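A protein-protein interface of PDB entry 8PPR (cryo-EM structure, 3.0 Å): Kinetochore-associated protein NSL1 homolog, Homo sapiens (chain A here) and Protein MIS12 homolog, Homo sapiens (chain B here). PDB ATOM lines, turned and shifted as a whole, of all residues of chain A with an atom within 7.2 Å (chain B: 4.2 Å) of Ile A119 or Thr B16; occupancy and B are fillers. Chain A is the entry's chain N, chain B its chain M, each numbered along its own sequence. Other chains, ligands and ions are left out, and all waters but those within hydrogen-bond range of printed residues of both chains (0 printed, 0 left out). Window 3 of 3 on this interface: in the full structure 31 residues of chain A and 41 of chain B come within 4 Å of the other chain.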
ATOM      1  N   ASP A 113       1.316 -29.453   1.975  1.00  0.00           N
ATOM      2  CA  ASP A 113       1.685 -30.571   1.115  1.00  0.00           C
ATOM      3  C   ASP A 113       0.778 -30.643  -0.105  1.00  0.00           C
ATOM      4  O   ASP A 113       1.248 -30.871  -1.226  1.00  0.00           O
ATOM      5  CB  ASP A 113       1.636 -31.877   1.907  1.00  0.00           C
ATOM      6  CG  ASP A 113       2.040 -33.080   1.076  1.00  0.00           C
ATOM      7  OD1 ASP A 113       2.798 -32.904   0.099  1.00  0.00           O
ATOM      8  OD2 ASP A 113       1.601 -34.201   1.402  1.00  0.00           O
ATOM      9  N   GLN A 114      -0.528 -30.442   0.094  1.00  0.00           N
ATOM     10  CA  GLN A 114      -1.460 -30.431  -1.029  1.00  0.00           C
ATOM     11  C   GLN A 114      -1.149 -29.296  -1.993  1.00  0.00           C
ATOM     12  O   GLN A 114      -1.198 -29.479  -3.214  1.00  0.00           O
ATOM     13  CB  GLN A 114      -2.894 -30.318  -0.514  1.00  0.00           C
ATOM     14  CG  GLN A 114      -3.943 -30.341  -1.610  1.00  0.00           C
ATOM     15  CD  GLN A 114      -4.002 -31.672  -2.328  1.00  0.00           C
ATOM     16  OE1 GLN A 114      -3.921 -32.730  -1.705  1.00  0.00           O
ATOM     17  NE2 GLN A 114      -4.143 -31.626  -3.648  1.00  0.00           N
ATOM     18  N   PHE A 115      -0.836 -28.113  -1.463  1.00  0.00           N
ATOM     19  CA  PHE A 115      -0.505 -26.979  -2.320  1.00  0.00           C
ATOM     20  C   PHE A 115       0.742 -27.262  -3.147  1.00  0.00           C
ATOM     21  O   PHE A 115       0.770 -27.009  -4.354  1.00  0.00           O
ATOM     22  CB  PHE A 115      -0.316 -25.723  -1.471  1.00  0.00           C
ATOM     23  CG  PHE A 115       0.065 -24.508  -2.267  1.00  0.00           C
ATOM     24  CD1 PHE A 115      -0.877 -23.839  -3.029  1.00  0.00           C
ATOM     25  CD2 PHE A 115       1.367 -24.037  -2.255  1.00  0.00           C
ATOM     26  CE1 PHE A 115      -0.529 -22.722  -3.764  1.00  0.00           C
ATOM     27  CE2 PHE A 115       1.721 -22.921  -2.988  1.00  0.00           C
ATOM     28  CZ  PHE A 115       0.771 -22.262  -3.743  1.00  0.00           C
ATOM     29  N   ASP A 116       1.784 -27.800  -2.511  1.00  0.00           N
ATOM     30  CA  ASP A 116       3.006 -28.112  -3.245  1.00  0.00           C
ATOM     31  C   ASP A 116       2.758 -29.188  -4.295  1.00  0.00           C
ATOM     32  O   ASP A 116       3.264 -29.095  -5.423  1.00  0.00           O
ATOM     33  CB  ASP A 116       4.099 -28.547  -2.272  1.00  0.00           C
ATOM     34  CG  ASP A 116       5.492 -28.354  -2.832  1.00  0.00           C
ATOM     35  OD1 ASP A 116       5.673 -28.527  -4.055  1.00  0.00           O
ATOM     36  OD2 ASP A 116       6.407 -28.026  -2.049  1.00  0.00           O
ATOM     37  N   GLU A 117       1.980 -30.214  -3.944  1.00  0.00           N
ATOM     38  CA  GLU A 117       1.691 -31.278  -4.895  1.00  0.00           C
ATOM     39  C   GLU A 117       0.903 -30.750  -6.086  1.00  0.00           C
ATOM     40  O   GLU A 117       1.169 -31.132  -7.230  1.00  0.00           O
ATOM     41  CB  GLU A 117       0.929 -32.407  -4.202  1.00  0.00           C
ATOM     42  CG  GLU A 117       0.689 -33.615  -5.085  1.00  0.00           C
ATOM     43  CD  GLU A 117       1.976 -34.321  -5.464  1.00  0.00           C
ATOM     44  OE1 GLU A 117       2.935 -34.282  -4.662  1.00  0.00           O
ATOM     45  OE2 GLU A 117       2.033 -34.911  -6.563  1.00  0.00           O
ATOM     46  N   ILE A 118      -0.068 -29.867  -5.840  1.00  0.00           N
ATOM     47  CA  ILE A 118      -0.847 -29.322  -6.945  1.00  0.00           C
ATOM     48  C   ILE A 118       0.007 -28.389  -7.796  1.00  0.00           C
ATOM     49  O   ILE A 118      -0.159 -28.337  -9.019  1.00  0.00           O
ATOM     50  CB  ILE A 118      -2.129 -28.637  -6.428  1.00  0.00           C
ATOM     51  CG1 ILE A 118      -3.200 -28.632  -7.520  1.00  0.00           C
ATOM     52  CG2 ILE A 118      -1.868 -27.216  -5.959  1.00  0.00           C
ATOM     53  CD1 ILE A 118      -3.580 -30.011  -7.994  1.00  0.00           C
ATOM     54  N   ILE A 119       0.947 -27.663  -7.182  1.00  0.00           N
ATOM     55  CA  ILE A 119       1.881 -26.850  -7.958  1.00  0.00           C
ATOM     56  C   ILE A 119       2.690 -27.732  -8.897  1.00  0.00           C
ATOM     57  O   ILE A 119       2.797 -27.460 -10.100  1.00  0.00           O
ATOM     58  CB  ILE A 119       2.803 -26.045  -7.023  1.00  0.00           C
ATOM     59  CG1 ILE A 119       2.019 -24.964  -6.280  1.00  0.00           C
ATOM     60  CG2 ILE A 119       3.956 -25.434  -7.806  1.00  0.00           C
ATOM     61  CD1 ILE A 119       1.552 -23.846  -7.171  1.00  0.00           C
ATOM     62  N   VAL A 120       3.262 -28.809  -8.358  1.00  0.00           N
ATOM     63  CA  VAL A 120       4.077 -29.705  -9.174  1.00  0.00           C
ATOM     64  C   VAL A 120       3.237 -30.321 -10.286  1.00  0.00           C
ATOM     65  O   VAL A 120       3.662 -30.385 -11.447  1.00  0.00           O
ATOM     66  CB  VAL A 120       4.731 -30.780  -8.288  1.00  0.00           C
ATOM     67  CG1 VAL A 120       5.221 -31.945  -9.133  1.00  0.00           C
ATOM     68  CG2 VAL A 120       5.872 -30.178  -7.481  1.00  0.00           C
ATOM     69  N   ASP A 121       2.027 -30.772  -9.950  1.00  0.00           N
ATOM     70  CA  ASP A 121       1.171 -31.421 -10.936  1.00  0.00           C
ATOM     71  C   ASP A 121       0.781 -30.464 -12.052  1.00  0.00           C
ATOM     72  O   ASP A 121       0.826 -30.830 -13.233  1.00  0.00           O
ATOM     73  CB  ASP A 121      -0.078 -31.978 -10.254  1.00  0.00           C
ATOM     74  CG  ASP A 121      -1.140 -32.400 -11.248  1.00  0.00           C
ATOM     75  OD1 ASP A 121      -0.791 -33.079 -12.237  1.00  0.00           O
ATOM     76  OD2 ASP A 121      -2.320 -32.048 -11.044  1.00  0.00           O
ATOM     77  N   ILE A 122       0.388 -29.237 -11.706  1.00  0.00           N
ATOM     78  CA  ILE A 122      -0.028 -28.295 -12.737  1.00  0.00           C
ATOM     79  C   ILE A 122       1.162 -27.857 -13.579  1.00  0.00           C
ATOM     80  O   ILE A 122       1.022 -27.625 -14.786  1.00  0.00           O
ATOM     81  CB  ILE A 122      -0.775 -27.101 -12.109  1.00  0.00           C
ATOM     82  CG1 ILE A 122      -1.659 -26.427 -13.158  1.00  0.00           C
ATOM     83  CG2 ILE A 122       0.189 -26.102 -11.480  1.00  0.00           C
ATOM     84  CD1 ILE A 122      -2.770 -27.318 -13.666  1.00  0.00           C
ATOM     85  N   ALA A 123       2.353 -27.758 -12.980  1.00  0.00           N
ATOM     86  CA  ALA A 123       3.542 -27.440 -13.760  1.00  0.00           C
ATOM     87  C   ALA A 123       3.846 -28.545 -14.764  1.00  0.00           C
ATOM     88  O   ALA A 123       4.137 -28.276 -15.938  1.00  0.00           O
ATOM     89  CB  ALA A 123       4.728 -27.217 -12.822  1.00  0.00           C
ATOM     90  N   THR A 124       3.768 -29.802 -14.319  1.00  0.00           N
ATOM     91  CA  THR A 124       3.984 -30.921 -15.230  1.00  0.00           C
ATOM     92  C   THR A 124       2.933 -30.947 -16.329  1.00  0.00           C
ATOM     93  O   THR A 124       3.245 -31.233 -17.490  1.00  0.00           O
ATOM     94  CB  THR A 124       3.980 -32.239 -14.457  1.00  0.00           C
ATOM     95  OG1 THR A 124       2.754 -32.361 -13.724  1.00  0.00           O
ATOM     96  CG2 THR A 124       5.158 -32.301 -13.497  1.00  0.00           C
ATOM     97  N   LYS A 125       1.678 -30.660 -15.979  1.00  0.00           N
ATOM     98  CA  LYS A 125       0.621 -30.619 -16.983  1.00  0.00           C
ATOM     99  C   LYS A 125       0.899 -29.543 -18.023  1.00  0.00           C
ATOM    100  O   LYS A 125       0.784 -29.791 -19.229  1.00  0.00           O
ATOM    101  CB  LYS A 125      -0.728 -30.380 -16.308  1.00  0.00           C
ATOM    102  CG  LYS A 125      -1.279 -31.599 -15.592  1.00  0.00           C
ATOM    103  CD  LYS A 125      -2.696 -31.359 -15.106  1.00  0.00           C
ATOM    104  CE  LYS A 125      -3.206 -32.538 -14.294  1.00  0.00           C
ATOM    105  NZ  LYS A 125      -2.964 -33.833 -14.983  1.00  0.00           N
ATOM    106  N   ARG A 126       1.295 -28.352 -17.572  1.00  0.00           N
ATOM    107  CA  ARG A 126       1.620 -27.274 -18.499  1.00  0.00           C
ATOM    108  C   ARG A 126       2.773 -27.664 -19.410  1.00  0.00           C
ATOM    109  O   ARG A 126       2.771 -27.339 -20.602  1.00  0.00           O
ATOM    110  CB  ARG A 126       1.969 -26.005 -17.725  1.00  0.00           C
ATOM    111  CG  ARG A 126       0.782 -25.133 -17.374  1.00  0.00           C
ATOM    112  CD  ARG A 126       1.211 -24.012 -16.448  1.00  0.00           C
ATOM    113  NE  ARG A 126       0.079 -23.382 -15.781  1.00  0.00           N
ATOM    114  CZ  ARG A 126       0.188 -22.559 -14.748  1.00  0.00           C
ATOM    115  NH1 ARG A 126       1.366 -22.242 -14.238  1.00  0.00           N
ATOM    116  NH2 ARG A 126      -0.914 -22.041 -14.211  1.00  0.00           N
ATOM    117  N   PRO B   5       3.435 -18.436  -5.607  1.00  0.00           N
ATOM    118  CA  PRO B   5       3.226 -19.803  -6.111  1.00  0.00           C
ATOM    119  C   PRO B   5       4.456 -20.397  -6.775  1.00  0.00           C
ATOM    120  O   PRO B   5       4.685 -21.608  -6.655  1.00  0.00           O
ATOM    121  CB  PRO B   5       2.065 -19.638  -7.103  1.00  0.00           C
ATOM    122  CG  PRO B   5       2.067 -18.188  -7.468  1.00  0.00           C
ATOM    123  CD  PRO B   5       2.526 -17.466  -6.239  1.00  0.00           C
ATOM    124  N   ALA B  10       8.802 -23.914 -10.648  1.00  0.00           N
ATOM    125  CA  ALA B  10       8.506 -25.328 -10.443  1.00  0.00           C
ATOM    126  C   ALA B  10       8.408 -26.065 -11.771  1.00  0.00           C
ATOM    127  O   ALA B  10       8.842 -27.217 -11.883  1.00  0.00           O
ATOM    128  CB  ALA B  10       7.215 -25.485  -9.641  1.00  0.00           C
ATOM    129  N   PHE B  15      10.277 -29.111  -9.444  1.00  0.00           N
ATOM    130  CA  PHE B  15       9.897 -29.137  -8.040  1.00  0.00           C
ATOM    131  C   PHE B  15       9.771 -27.710  -7.528  1.00  0.00           C
ATOM    132  O   PHE B  15      10.345 -26.773  -8.089  1.00  0.00           O
ATOM    133  CB  PHE B  15      10.914 -29.912  -7.192  1.00  0.00           C
ATOM    134  CG  PHE B  15      12.317 -29.387  -7.302  1.00  0.00           C
ATOM    135  CD1 PHE B  15      13.172 -29.861  -8.282  1.00  0.00           C
ATOM    136  CD2 PHE B  15      12.778 -28.415  -6.429  1.00  0.00           C
ATOM    137  CE1 PHE B  15      14.461 -29.378  -8.388  1.00  0.00           C
ATOM    138  CE2 PHE B  15      14.065 -27.928  -6.529  1.00  0.00           C
ATOM    139  CZ  PHE B  15      14.909 -28.410  -7.511  1.00  0.00           C
ATOM    140  N   THR B  16       9.014 -27.557  -6.453  1.00  0.00           N
ATOM    141  CA  THR B  16       8.887 -26.256  -5.811  1.00  0.00           C
ATOM    142  C   THR B  16      10.179 -25.919  -5.076  1.00  0.00           C
ATOM    143  O   THR B  16      10.697 -26.758  -4.332  1.00  0.00           O
ATOM    144  CB  THR B  16       7.714 -26.244  -4.836  1.00  0.00           C
ATOM    145  OG1 THR B  16       6.487 -26.377  -5.563  1.00  0.00           O
ATOM    146  CG2 THR B  16       7.687 -24.947  -4.043  1.00  0.00           C
ATOM    147  N   PRO B  17      10.734 -24.720  -5.268  1.00  0.00           N
ATOM    148  CA  PRO B  17      11.961 -24.359  -4.540  1.00  0.00           C
ATOM    149  C   PRO B  17      11.804 -24.410  -3.032  1.00  0.00           C
ATOM    150  O   PRO B  17      12.775 -24.717  -2.326  1.00  0.00           O
ATOM    151  CB  PRO B  17      12.248 -22.932  -5.030  1.00  0.00           C
ATOM    152  CG  PRO B  17      11.557 -22.838  -6.351  1.00  0.00           C
ATOM    153  CD  PRO B  17      10.324 -23.677  -6.222  1.00  0.00           C
ATOM    154  N   GLN B  18      10.609 -24.117  -2.513  1.00  0.00           N
ATOM    155  CA  GLN B  18      10.395 -24.200  -1.072  1.00  0.00           C
ATOM    156  C   GLN B  18      10.624 -25.614  -0.561  1.00  0.00           C
ATOM    157  O   GLN B  18      11.112 -25.803   0.557  1.00  0.00           O
ATOM    158  CB  GLN B  18       8.988 -23.723  -0.715  1.00  0.00           C
ATOM    159  CG  GLN B  18       8.802 -22.222  -0.807  1.00  0.00           C
ATOM    160  CD  GLN B  18       7.382 -21.791  -0.504  1.00  0.00           C
ATOM    161  OE1 GLN B  18       6.498 -22.623  -0.303  1.00  0.00           O
ATOM    162  NE2 GLN B  18       7.157 -20.483  -0.468  1.00  0.00           N
ATOM    163  N   THR B  19      10.283 -26.621  -1.369  1.00  0.00           N
ATOM    164  CA  THR B  19      10.491 -28.006  -0.957  1.00  0.00           C
ATOM    165  C   THR B  19      11.969 -28.289  -0.715  1.00  0.00           C
ATOM    166  O   THR B  19      12.352 -28.826   0.331  1.00  0.00           O
ATOM    167  CB  THR B  19       9.932 -28.956  -2.015  1.00  0.00           C
ATOM    168  OG1 THR B  19       8.533 -28.703  -2.194  1.00  0.00           O
ATOM    169  CG2 THR B  19      10.131 -30.401  -1.589  1.00  0.00           C
ATOM    170  N   CYS B  20      12.819 -27.927  -1.677  1.00  0.00           N
ATOM    171  CA  CYS B  20      14.249 -28.166  -1.518  1.00  0.00           C
ATOM    172  C   CYS B  20      14.850 -27.293  -0.422  1.00  0.00           C
ATOM    173  O   CYS B  20      15.740 -27.747   0.303  1.00  0.00           O
ATOM    174  CB  CYS B  20      14.961 -27.958  -2.855  1.00  0.00           C
ATOM    175  SG  CYS B  20      15.249 -26.245  -3.325  1.00  0.00           S
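Hydrophobic or aromatic side chains of chain A that line the printed part of chain B: Ile A119 and Ala A123.
Hydrophobic or aromatic side chains of chain B within 4 Å of the printed part of chain A: Ala B10.
Among the printed residues, 6 pairs touch across the chains.
Among the printed residues, no Asp or Glu carboxylate lies within 4 Å of a Lys or Arg side-chain nitrogen of the other chain.
The side-chain carboxylate (OD1) of Asp A116 sits at hydrogen-bond distance from the side-chain hydroxyl (OG1) of Thr B16 (2.7 Å).
The side-chain hydroxyl (OG1) of Thr B19 sits close to the side-chain carboxylate (OD1) of Asp A116 (3.4 Å).
Ile A119 touches three residues of chain B.
Of chain A, only Asp A116 and Ile A119 come within 4 Å of Thr B16.
Of the printed residues of chain A, Ala B10 touches Ile A119 (3.7 Å) and Ala A123 (3.997 Å).
Of the printed residues of chain B, Asp A116 touches Thr B16 (2.7 Å) and Thr B19 (2.2 Å).
Printed residues of chain A within 4 Å of Thr B19: Asp A116 (2.2 Å).
Of the printed residues of chain B, Ala A123 touches Ala B10.
Printed residues of chain A within 4 Å of Pro B5: Ile A119 (3.9 Å).
Ile A122 touches none of the printed residues of chain B.
The nearest printed residue of chain B that does not touch Ile A119 is Phe B15 (6.3 Å).
The nearest printed residue of chain A that does not touch Thr B19 is Val A120 (6.1 Å).
The backbone carbonyl oxygen of Ala B10 is in hydrogen-bond range of the backbone NH of Phe B15.
Ile A119 touches Pro B5 (CD1 to O, 3.9 Å).
CG2 of Ile A119 touches CB of Ala B10, at 3.7 Å.
Ile A119 touches Thr B16 (CG2 to OG1, 3.5 Å).
C of Ala B10 touches CB of Ala A123, 3.997 Å away.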
